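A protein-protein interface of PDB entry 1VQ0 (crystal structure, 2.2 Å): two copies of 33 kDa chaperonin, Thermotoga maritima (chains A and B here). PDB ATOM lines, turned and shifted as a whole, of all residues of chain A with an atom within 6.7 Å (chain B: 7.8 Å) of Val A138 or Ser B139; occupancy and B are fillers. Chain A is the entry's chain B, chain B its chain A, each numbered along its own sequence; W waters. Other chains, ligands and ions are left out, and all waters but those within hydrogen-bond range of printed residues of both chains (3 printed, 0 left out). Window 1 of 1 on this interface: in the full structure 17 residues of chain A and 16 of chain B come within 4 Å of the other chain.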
ATOM      1  N   ARG A 126     -21.287 -30.041 -27.964  1.00  0.00           N
ATOM      2  CA  ARG A 126     -21.316 -30.379 -26.532  1.00  0.00           C
ATOM      3  C   ARG A 126     -19.910 -30.638 -25.997  1.00  0.00           C
ATOM      4  O   ARG A 126     -19.068 -31.147 -26.728  1.00  0.00           O
ATOM      5  CB  ARG A 126     -22.205 -31.638 -26.296  1.00  0.00           C
ATOM      6  CG  ARG A 126     -23.585 -31.314 -26.262  1.00  0.00           C
ATOM      7  CD  ARG A 126     -24.493 -32.449 -25.900  1.00  0.00           C
ATOM      8  NE  ARG A 126     -24.475 -33.392 -26.981  1.00  0.00           N
ATOM      9  CZ  ARG A 126     -25.349 -33.496 -27.957  1.00  0.00           C
ATOM     10  NH1 ARG A 126     -26.406 -32.730 -28.027  1.00  0.00           N
ATOM     11  NH2 ARG A 126     -25.135 -34.428 -28.873  1.00  0.00           N
ATOM     12  N   VAL A 127     -19.654 -30.180 -24.768  1.00  0.00           N
ATOM     13  CA  VAL A 127     -18.470 -30.510 -24.036  1.00  0.00           C
ATOM     14  C   VAL A 127     -18.947 -31.109 -22.728  1.00  0.00           C
ATOM     15  O   VAL A 127     -19.794 -30.537 -22.034  1.00  0.00           O
ATOM     16  CB  VAL A 127     -17.518 -29.334 -23.872  1.00  0.00           C
ATOM     17  CG1 VAL A 127     -16.312 -29.728 -22.904  1.00  0.00           C
ATOM     18  CG2 VAL A 127     -17.008 -28.919 -25.270  1.00  0.00           C
ATOM     19  N   VAL A 128     -18.481 -32.327 -22.477  1.00  0.00           N
ATOM     20  CA  VAL A 128     -18.800 -33.126 -21.262  1.00  0.00           C
ATOM     21  C   VAL A 128     -17.526 -33.146 -20.472  1.00  0.00           C
ATOM     22  O   VAL A 128     -16.507 -33.584 -20.970  1.00  0.00           O
ATOM     23  CB  VAL A 128     -19.170 -34.586 -21.606  1.00  0.00           C
ATOM     24  CG1 VAL A 128     -19.552 -35.348 -20.390  1.00  0.00           C
ATOM     25  CG2 VAL A 128     -20.273 -34.579 -22.640  1.00  0.00           C
ATOM     26  N   ARG A 129     -17.585 -32.586 -19.282  1.00  0.00           N
ATOM     27  CA  ARG A 129     -16.521 -32.655 -18.295  1.00  0.00           C
ATOM     28  C   ARG A 129     -16.862 -33.635 -17.136  1.00  0.00           C
ATOM     29  O   ARG A 129     -17.626 -33.346 -16.217  1.00  0.00           O
ATOM     30  CB  ARG A 129     -16.252 -31.309 -17.727  1.00  0.00           C
ATOM     31  CG  ARG A 129     -15.634 -30.360 -18.749  1.00  0.00           C
ATOM     32  CD  ARG A 129     -14.243 -30.068 -18.336  1.00  0.00           C
ATOM     33  NE  ARG A 129     -14.207 -28.843 -17.624  1.00  0.00           N
ATOM     34  CZ  ARG A 129     -13.245 -28.402 -16.827  1.00  0.00           C
ATOM     35  NH1 ARG A 129     -12.169 -29.066 -16.459  1.00  0.00           N
ATOM     36  NH2 ARG A 129     -13.444 -27.250 -16.304  1.00  0.00           N
ATOM     37  N   PRO A 136     -21.482 -35.833 -14.892  1.00  0.00           N
ATOM     38  CA  PRO A 136     -20.567 -34.830 -15.473  1.00  0.00           C
ATOM     39  C   PRO A 136     -21.220 -33.460 -15.780  1.00  0.00           C
ATOM     40  O   PRO A 136     -22.442 -33.344 -15.816  1.00  0.00           O
ATOM     41  CB  PRO A 136     -20.149 -35.515 -16.783  1.00  0.00           C
ATOM     42  CG  PRO A 136     -21.402 -36.179 -17.205  1.00  0.00           C
ATOM     43  CD  PRO A 136     -21.965 -36.760 -15.927  1.00  0.00           C
ATOM     44  N   PHE A 137     -20.385 -32.418 -15.901  1.00  0.00           N
ATOM     45  CA  PHE A 137     -20.849 -31.123 -16.326  1.00  0.00           C
ATOM     46  C   PHE A 137     -21.015 -31.265 -17.789  1.00  0.00           C
ATOM     47  O   PHE A 137     -20.201 -31.905 -18.431  1.00  0.00           O
ATOM     48  CB  PHE A 137     -19.814 -30.061 -16.000  1.00  0.00           C
ATOM     49  CG  PHE A 137     -19.591 -29.898 -14.541  1.00  0.00           C
ATOM     50  CD1 PHE A 137     -20.449 -29.150 -13.774  1.00  0.00           C
ATOM     51  CD2 PHE A 137     -18.507 -30.533 -13.904  1.00  0.00           C
ATOM     52  CE1 PHE A 137     -20.291 -29.059 -12.380  1.00  0.00           C
ATOM     53  CE2 PHE A 137     -18.320 -30.421 -12.507  1.00  0.00           C
ATOM     54  CZ  PHE A 137     -19.215 -29.669 -11.754  1.00  0.00           C
ATOM     55  N   VAL A 138     -22.109 -30.796 -18.337  1.00  0.00           N
ATOM     56  CA  VAL A 138     -22.309 -30.822 -19.804  1.00  0.00           C
ATOM     57  C   VAL A 138     -22.722 -29.402 -20.220  1.00  0.00           C
ATOM     58  O   VAL A 138     -23.597 -28.786 -19.594  1.00  0.00           O
ATOM     59  CB  VAL A 138     -23.401 -31.730 -20.292  1.00  0.00           C
ATOM     60  CG1 VAL A 138     -23.389 -31.786 -21.786  1.00  0.00           C
ATOM     61  CG2 VAL A 138     -23.337 -33.147 -19.718  1.00  0.00           C
ATOM     62  N   SER A 139     -22.077 -28.889 -21.267  1.00  0.00           N
ATOM     63  CA  SER A 139     -22.402 -27.585 -21.792  1.00  0.00           C
ATOM     64  C   SER A 139     -22.633 -27.695 -23.291  1.00  0.00           C
ATOM     65  O   SER A 139     -21.804 -28.253 -23.986  1.00  0.00           O
ATOM     66  CB  SER A 139     -21.304 -26.578 -21.364  1.00  0.00           C
ATOM     67  OG  SER A 139     -21.318 -25.401 -22.154  1.00  0.00           O
ATOM     68  N   GLN A 140     -23.761 -27.182 -23.795  1.00  0.00           N
ATOM     69  CA  GLN A 140     -24.061 -27.249 -25.213  1.00  0.00           C
ATOM     70  C   GLN A 140     -24.259 -25.874 -25.841  1.00  0.00           C
ATOM     71  O   GLN A 140     -24.943 -25.051 -25.289  1.00  0.00           O
ATOM     72  CB  GLN A 140     -25.292 -28.162 -25.489  1.00  0.00           C
ATOM     73  CG  GLN A 140     -25.785 -28.146 -26.888  1.00  0.00           C
ATOM     74  CD  GLN A 140     -27.105 -28.875 -27.058  1.00  0.00           C
ATOM     75  OE1 GLN A 140     -27.241 -30.035 -26.612  1.00  0.00           O
ATOM     76  NE2 GLN A 140     -28.104 -28.185 -27.721  1.00  0.00           N
ATOM     77  N   TYR A 155     -17.338 -22.191 -27.983  1.00  0.00           N
ATOM     78  CA  TYR A 155     -17.661 -22.872 -26.707  1.00  0.00           C
ATOM     79  C   TYR A 155     -16.826 -22.207 -25.554  1.00  0.00           C
ATOM     80  O   TYR A 155     -17.388 -21.778 -24.509  1.00  0.00           O
ATOM     81  CB  TYR A 155     -17.444 -24.385 -26.777  1.00  0.00           C
ATOM     82  CG  TYR A 155     -17.280 -24.960 -25.389  1.00  0.00           C
ATOM     83  CD1 TYR A 155     -18.400 -25.279 -24.587  1.00  0.00           C
ATOM     84  CD2 TYR A 155     -16.004 -25.102 -24.834  1.00  0.00           C
ATOM     85  CE1 TYR A 155     -18.255 -25.785 -23.281  1.00  0.00           C
ATOM     86  CE2 TYR A 155     -15.840 -25.556 -23.511  1.00  0.00           C
ATOM     87  CZ  TYR A 155     -16.949 -25.877 -22.724  1.00  0.00           C
ATOM     88  OH  TYR A 155     -16.719 -26.303 -21.413  1.00  0.00           O
ATOM     89  N   THR B  73     -35.219 -21.864 -19.155  1.00  0.00           N
ATOM     90  CA  THR B  73     -35.884 -23.061 -18.629  1.00  0.00           C
ATOM     91  C   THR B  73     -34.991 -23.818 -17.633  1.00  0.00           C
ATOM     92  O   THR B  73     -33.853 -24.237 -17.958  1.00  0.00           O
ATOM     93  CB  THR B  73     -36.248 -24.018 -19.750  1.00  0.00           C
ATOM     94  OG1 THR B  73     -37.025 -23.358 -20.758  1.00  0.00           O
ATOM     95  CG2 THR B  73     -37.108 -25.195 -19.259  1.00  0.00           C
ATOM     96  N   ASP B  75     -34.723 -27.306 -15.867  1.00  0.00           N
ATOM     97  CA  ASP B  75     -35.104 -28.687 -16.042  1.00  0.00           C
ATOM     98  C   ASP B  75     -34.271 -29.579 -15.057  1.00  0.00           C
ATOM     99  O   ASP B  75     -33.088 -29.818 -15.244  1.00  0.00           O
ATOM    100  CB  ASP B  75     -34.832 -29.082 -17.493  1.00  0.00           C
ATOM    101  CG  ASP B  75     -35.122 -30.503 -17.761  1.00  0.00           C
ATOM    102  OD1 ASP B  75     -35.838 -31.105 -16.976  1.00  0.00           O
ATOM    103  OD2 ASP B  75     -34.680 -31.114 -18.744  1.00  0.00           O
ATOM    104  N   VAL B 124     -29.875 -34.452 -11.848  1.00  0.00           N
ATOM    105  CA  VAL B 124     -29.143 -33.349 -12.480  1.00  0.00           C
ATOM    106  C   VAL B 124     -30.051 -32.105 -12.639  1.00  0.00           C
ATOM    107  O   VAL B 124     -31.277 -32.183 -12.640  1.00  0.00           O
ATOM    108  CB  VAL B 124     -28.581 -33.755 -13.924  1.00  0.00           C
ATOM    109  CG1 VAL B 124     -27.792 -34.949 -13.855  1.00  0.00           C
ATOM    110  CG2 VAL B 124     -29.679 -33.954 -14.967  1.00  0.00           C
ATOM    111  N   LEU B 125     -29.401 -30.962 -12.783  1.00  0.00           N
ATOM    112  CA  LEU B 125     -30.083 -29.736 -13.102  1.00  0.00           C
ATOM    113  C   LEU B 125     -29.541 -29.159 -14.415  1.00  0.00           C
ATOM    114  O   LEU B 125     -28.360 -29.072 -14.597  1.00  0.00           O
ATOM    115  CB  LEU B 125     -29.922 -28.762 -11.951  1.00  0.00           C
ATOM    116  CG  LEU B 125     -30.485 -27.341 -12.078  1.00  0.00           C
ATOM    117  CD1 LEU B 125     -30.575 -26.709 -10.674  1.00  0.00           C
ATOM    118  CD2 LEU B 125     -29.613 -26.508 -12.915  1.00  0.00           C
ATOM    119  N   ARG B 126     -30.468 -28.834 -15.310  1.00  0.00           N
ATOM    120  CA  ARG B 126     -30.257 -28.209 -16.609  1.00  0.00           C
ATOM    121  C   ARG B 126     -30.869 -26.824 -16.661  1.00  0.00           C
ATOM    122  O   ARG B 126     -31.943 -26.624 -16.149  1.00  0.00           O
ATOM    123  CB  ARG B 126     -30.897 -29.041 -17.746  1.00  0.00           C
ATOM    124  CG  ARG B 126     -30.098 -30.177 -18.098  1.00  0.00           C
ATOM    125  CD  ARG B 126     -30.533 -31.010 -19.284  1.00  0.00           C
ATOM    126  NE  ARG B 126     -31.719 -31.718 -18.941  1.00  0.00           N
ATOM    127  CZ  ARG B 126     -31.807 -32.950 -18.497  1.00  0.00           C
ATOM    128  NH1 ARG B 126     -30.766 -33.709 -18.350  1.00  0.00           N
ATOM    129  NH2 ARG B 126     -33.002 -33.432 -18.237  1.00  0.00           N
ATOM    130  N   VAL B 127     -30.146 -25.899 -17.285  1.00  0.00           N
ATOM    131  CA  VAL B 127     -30.654 -24.578 -17.662  1.00  0.00           C
ATOM    132  C   VAL B 127     -30.497 -24.390 -19.165  1.00  0.00           C
ATOM    133  O   VAL B 127     -29.382 -24.478 -19.716  1.00  0.00           O
ATOM    134  CB  VAL B 127     -30.039 -23.464 -16.844  1.00  0.00           C
ATOM    135  CG1 VAL B 127     -30.479 -22.057 -17.352  1.00  0.00           C
ATOM    136  CG2 VAL B 127     -30.411 -23.686 -15.373  1.00  0.00           C
ATOM    137  N   VAL B 128     -31.644 -24.179 -19.806  1.00  0.00           N
ATOM    138  CA  VAL B 128     -31.768 -23.903 -21.257  1.00  0.00           C
ATOM    139  C   VAL B 128     -32.001 -22.417 -21.457  1.00  0.00           C
ATOM    140  O   VAL B 128     -32.915 -21.841 -20.880  1.00  0.00           O
ATOM    141  CB  VAL B 128     -32.920 -24.682 -21.866  1.00  0.00           C
ATOM    142  CG1 VAL B 128     -32.971 -24.563 -23.334  1.00  0.00           C
ATOM    143  CG2 VAL B 128     -32.770 -26.157 -21.472  1.00  0.00           C
ATOM    144  N   ARG B 129     -31.122 -21.798 -22.229  1.00  0.00           N
ATOM    145  CA  ARG B 129     -31.232 -20.393 -22.553  1.00  0.00           C
ATOM    146  C   ARG B 129     -31.546 -20.253 -24.040  1.00  0.00           C
ATOM    147  O   ARG B 129     -30.732 -20.490 -24.907  1.00  0.00           O
ATOM    148  CB  ARG B 129     -29.962 -19.692 -22.214  1.00  0.00           C
ATOM    149  CG  ARG B 129     -29.805 -19.454 -20.729  1.00  0.00           C
ATOM    150  CD  ARG B 129     -29.929 -17.943 -20.484  1.00  0.00           C
ATOM    151  NE  ARG B 129     -28.663 -17.358 -20.296  1.00  0.00           N
ATOM    152  CZ  ARG B 129     -28.346 -16.076 -20.351  1.00  0.00           C
ATOM    153  NH1 ARG B 129     -29.121 -15.066 -20.681  1.00  0.00           N
ATOM    154  NH2 ARG B 129     -27.120 -15.805 -20.112  1.00  0.00           N
ATOM    155  N   PRO B 136     -30.695 -23.507 -28.571  1.00  0.00           N
ATOM    156  CA  PRO B 136     -30.419 -22.812 -27.313  1.00  0.00           C
ATOM    157  C   PRO B 136     -29.087 -23.212 -26.675  1.00  0.00           C
ATOM    158  O   PRO B 136     -28.480 -24.205 -27.080  1.00  0.00           O
ATOM    159  CB  PRO B 136     -31.583 -23.297 -26.413  1.00  0.00           C
ATOM    160  CG  PRO B 136     -31.861 -24.637 -26.881  1.00  0.00           C
ATOM    161  CD  PRO B 136     -31.599 -24.647 -28.347  1.00  0.00           C
ATOM    162  N   PHE B 137     -28.618 -22.384 -25.746  1.00  0.00           N
ATOM    163  CA  PHE B 137     -27.561 -22.755 -24.824  1.00  0.00           C
ATOM    164  C   PHE B 137     -28.132 -23.677 -23.775  1.00  0.00           C
ATOM    165  O   PHE B 137     -29.261 -23.479 -23.282  1.00  0.00           O
ATOM    166  CB  PHE B 137     -26.923 -21.519 -24.174  1.00  0.00           C
ATOM    167  CG  PHE B 137     -26.342 -20.580 -25.166  1.00  0.00           C
ATOM    168  CD1 PHE B 137     -25.127 -20.829 -25.741  1.00  0.00           C
ATOM    169  CD2 PHE B 137     -27.049 -19.465 -25.586  1.00  0.00           C
ATOM    170  CE1 PHE B 137     -24.584 -19.974 -26.707  1.00  0.00           C
ATOM    171  CE2 PHE B 137     -26.506 -18.594 -26.565  1.00  0.00           C
ATOM    172  CZ  PHE B 137     -25.278 -18.868 -27.121  1.00  0.00           C
ATOM    173  N   VAL B 138     -27.406 -24.736 -23.495  1.00  0.00           N
ATOM    174  CA  VAL B 138     -27.824 -25.672 -22.435  1.00  0.00           C
ATOM    175  C   VAL B 138     -26.623 -25.992 -21.539  1.00  0.00           C
ATOM    176  O   VAL B 138     -25.524 -26.288 -22.020  1.00  0.00           O
ATOM    177  CB  VAL B 138     -28.344 -27.042 -22.929  1.00  0.00           C
ATOM    178  CG1 VAL B 138     -28.929 -27.847 -21.751  1.00  0.00           C
ATOM    179  CG2 VAL B 138     -29.314 -26.943 -24.086  1.00  0.00           C
ATOM    180  N   SER B 139     -26.858 -25.971 -20.236  1.00  0.00           N
ATOM    181  CA  SER B 139     -25.827 -26.252 -19.286  1.00  0.00           C
ATOM    182  C   SER B 139     -26.399 -27.179 -18.245  1.00  0.00           C
ATOM    183  O   SER B 139     -27.459 -26.930 -17.741  1.00  0.00           O
ATOM    184  CB  SER B 139     -25.250 -24.916 -18.764  1.00  0.00           C
ATOM    185  OG  SER B 139     -24.365 -25.132 -17.669  1.00  0.00           O
ATOM    186  N   GLN B 140     -25.692 -28.282 -17.965  1.00  0.00           N
ATOM    187  CA  GLN B 140     -26.081 -29.330 -17.019  1.00  0.00           C
ATOM    188  C   GLN B 140     -25.054 -29.545 -15.911  1.00  0.00           C
ATOM    189  O   GLN B 140     -23.869 -29.641 -16.140  1.00  0.00           O
ATOM    190  CB  GLN B 140     -26.347 -30.650 -17.735  1.00  0.00           C
ATOM    191  CG  GLN B 140     -26.834 -31.755 -16.796  1.00  0.00           C
ATOM    192  CD  GLN B 140     -26.975 -33.115 -17.465  1.00  0.00           C
ATOM    193  OE1 GLN B 140     -27.689 -33.213 -18.448  1.00  0.00           O
ATOM    194  NE2 GLN B 140     -26.252 -34.150 -16.967  1.00  0.00           N
ATOM    195  N   VAL B 141     -25.543 -29.569 -14.680  1.00  0.00           N
ATOM    196  CA  VAL B 141     -24.710 -29.781 -13.506  1.00  0.00           C
ATOM    197  C   VAL B 141     -25.359 -30.858 -12.620  1.00  0.00           C
ATOM    198  O   VAL B 141     -26.570 -30.997 -12.637  1.00  0.00           O
ATOM    199  CB  VAL B 141     -24.454 -28.447 -12.728  1.00  0.00           C
ATOM    200  CG1 VAL B 141     -23.719 -27.436 -13.581  1.00  0.00           C
ATOM    201  CG2 VAL B 141     -25.725 -27.874 -12.127  1.00  0.00           C
ATOM    202  N   PRO B 142     -24.571 -31.571 -11.821  1.00  0.00           N
ATOM    203  CA  PRO B 142     -25.130 -32.486 -10.889  1.00  0.00           C
ATOM    204  C   PRO B 142     -25.847 -31.733  -9.779  1.00  0.00           C
ATOM    205  O   PRO B 142     -25.504 -30.587  -9.519  1.00  0.00           O
ATOM    206  CB  PRO B 142     -23.939 -33.305 -10.380  1.00  0.00           C
ATOM    207  CG  PRO B 142     -22.698 -32.489 -10.763  1.00  0.00           C
ATOM    208  CD  PRO B 142     -23.126 -31.473 -11.725  1.00  0.00           C
ATOM    209  N   TYR B 155     -25.462 -23.996  -9.988  1.00  0.00           N
ATOM    210  CA  TYR B 155     -25.490 -23.748 -11.435  1.00  0.00           C
ATOM    211  C   TYR B 155     -24.844 -22.352 -11.700  1.00  0.00           C
ATOM    212  O   TYR B 155     -23.841 -22.202 -12.475  1.00  0.00           O
ATOM    213  CB  TYR B 155     -26.913 -23.826 -12.016  1.00  0.00           C
ATOM    214  CG  TYR B 155     -26.961 -23.108 -13.303  1.00  0.00           C
ATOM    215  CD1 TYR B 155     -26.557 -23.741 -14.490  1.00  0.00           C
ATOM    216  CD2 TYR B 155     -27.369 -21.751 -13.361  1.00  0.00           C
ATOM    217  CE1 TYR B 155     -26.537 -23.032 -15.718  1.00  0.00           C
ATOM    218  CE2 TYR B 155     -27.322 -21.026 -14.552  1.00  0.00           C
ATOM    219  CZ  TYR B 155     -26.924 -21.655 -15.744  1.00  0.00           C
ATOM    220  OH  TYR B 155     -26.848 -20.936 -16.923  1.00  0.00           O
ATOM    221  N   PHE B 156     -25.353 -21.340 -11.003  1.00  0.00           N
ATOM    222  CA  PHE B 156     -24.849 -19.982 -11.266  1.00  0.00           C
ATOM    223  C   PHE B 156     -23.352 -19.859 -10.960  1.00  0.00           C
ATOM    224  O   PHE B 156     -22.590 -19.404 -11.831  1.00  0.00           O
ATOM    225  CB  PHE B 156     -25.715 -18.882 -10.592  1.00  0.00           C
ATOM    226  CG  PHE B 156     -26.964 -18.544 -11.388  1.00  0.00           C
ATOM    227  CD1 PHE B 156     -26.875 -17.728 -12.515  1.00  0.00           C
ATOM    228  CD2 PHE B 156     -28.240 -19.041 -11.016  1.00  0.00           C
ATOM    229  CE1 PHE B 156     -28.040 -17.423 -13.274  1.00  0.00           C
ATOM    230  CE2 PHE B 156     -29.386 -18.744 -11.796  1.00  0.00           C
ATOM    231  CZ  PHE B 156     -29.282 -17.954 -12.908  1.00  0.00           C
ATOM    232  N   VAL B 158     -20.997 -22.161 -10.899  1.00  0.00           N
ATOM    233  CA  VAL B 158     -20.121 -22.967 -11.724  1.00  0.00           C
ATOM    234  C   VAL B 158     -20.293 -22.693 -13.213  1.00  0.00           C
ATOM    235  O   VAL B 158     -19.291 -22.515 -13.850  1.00  0.00           O
ATOM    236  CB  VAL B 158     -20.285 -24.479 -11.458  1.00  0.00           C
ATOM    237  CG1 VAL B 158     -19.545 -25.289 -12.547  1.00  0.00           C
ATOM    238  CG2 VAL B 158     -19.690 -24.844 -10.100  1.00  0.00           C
ATOM    239  N   SER B 159     -21.514 -22.703 -13.785  1.00  0.00           N
ATOM    240  CA  SER B 159     -21.642 -22.456 -15.212  1.00  0.00           C
ATOM    241  C   SER B 159     -21.562 -20.987 -15.606  1.00  0.00           C
ATOM    242  O   SER B 159     -21.088 -20.662 -16.677  1.00  0.00           O
ATOM    243  CB  SER B 159     -22.927 -23.009 -15.808  1.00  0.00           C
ATOM    244  OG  SER B 159     -23.281 -24.237 -15.209  1.00  0.00           O
ATOM    245  N   GLU B 160     -22.085 -20.098 -14.798  1.00  0.00           N
ATOM    246  CA  GLU B 160     -22.105 -18.687 -15.196  1.00  0.00           C
ATOM    247  C   GLU B 160     -21.076 -17.849 -14.482  1.00  0.00           C
ATOM    248  O   GLU B 160     -20.957 -16.649 -14.750  1.00  0.00           O
ATOM    249  CB  GLU B 160     -23.493 -18.102 -14.953  1.00  0.00           C
ATOM    250  CG  GLU B 160     -24.591 -18.747 -15.776  1.00  0.00           C
ATOM    251  CD  GLU B 160     -25.754 -17.821 -16.051  1.00  0.00           C
ATOM    252  OE1 GLU B 160     -25.600 -16.598 -15.855  1.00  0.00           O
ATOM    253  OE2 GLU B 160     -26.816 -18.345 -16.478  1.00  0.00           O
HETATM  254  O   HOH W   1     -22.031 -24.566 -19.173  1.00  0.00           O
HETATM  255  O   HOH W   2     -27.288 -25.661 -28.975  1.00  0.00           O
HETATM  256  O   HOH W   3     -24.901 -33.548 -14.548  1.00  0.00           O
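Among the printed residues, pairs that only touch across the chains: Phe A137 with Gln B140, Ser A139 with Val B138, Val A138 with Ser B139, Gln A140 with Phe B137, Phe A137 with Val B141, Phe A137 with Pro B142, Phe A137 with Val B158, Val A138 with Val B138 and Pro A136 with Gln B140.
The backbone carbonyl oxygen (O) of Val B141 is in hydrogen-bond range of the backbone NH (N) of Leu B125 (2.8 Å). The side-chain amide oxygen of Gln B140 sits at hydrogen-bond distance from the guanidinium group of Arg B126 (3.1 Å). The backbone NH (N) of Val B127 sits at hydrogen-bond distance from the backbone carbonyl oxygen (O) of Ser B139, 2.9 Å away. O of Phe B137 is in hydrogen-bond range of N of Arg B129 (2.7 Å). The guanidinium group (NH1) of Arg A126 sits at hydrogen-bond distance from the side-chain amide oxygen (OE1) of Gln A140. The backbone carbonyl oxygen (O) of Val A127 lies within hydrogen-bond range of the backbone NH (N) of Ser A139.
The backbone carbonyl oxygen (O) of Val B138 sits at hydrogen-bond distance from the backbone NH (N) of Gln A140 (2.7 Å). The backbone carbonyl oxygen of Val A138 is in hydrogen-bond range of the backbone NH of Gln B140, 2.7 Å away.
Along chain A the printed residues that touch a printed residue of chain B span positions 136 to 140.
Water W2 bridges the backbone carbonyl oxygen of Pro B136 and the side-chain amide nitrogen of Gln A140. Water W3 lies within hydrogen-bond range of the backbone carbonyl oxygen of Pro A136 (2.8 Å) and the side-chain amide nitrogen of Gln B140 (2.8 Å). Water W1 bridges OG of Ser B139 (2.8 Å) and OG of Ser A139 (3.2 Å).
Phe A137 touches Gln B140, and with the chains exchanged Gln A140 touches Phe B137. Val A138 touches its own counterpart, Val B138. Val A138 touches Ser B139, and with the chains exchanged Ser A139 touches Val B138. Val A138 touches Gln B140, and with the chains exchanged Gln A140 touches Val B138. Positions printed for both chains: 126, 127, 128, 129, 136, 137, 138, 139, 140 and 155. Of the 11 pairs that touch across the chains among the printed residues, 7 have their exchanged pair printed and touching as well.
Arg A129 touches none of the printed residues of chain B. Of the printed residues of chain B, Phe A137 touches Gln B140 (3.4 Å), Val B141 (3.7 Å), Pro B142 (3.8 Å) and Val B158 (3.8 Å). Of the printed residues of chain B, Gln A140 touches Phe B137 and Val B138. Of the printed residues of chain A, Phe B137 touches Gln A140. Printed residues of chain A within 4 Å of Val B138: Val A138, Ser A139 and Gln A140. Ser B139 touches just one residue of chain A: Val A138 (3.4 Å). Of the printed residues of chain A, Pro B142 touches Phe A137 (3.8 Å). Phe B156 touches none of the printed residues of chain A. The nearest residue of chain B that does not touch Val A138 is Val B141 (5.2 Å). The nearest residue of chain A that does not touch Ser B139 is Ser A139 (4.4 Å). The nearest printed residue of chain A that does not touch Val B141 is Pro A136 (4.8 Å).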
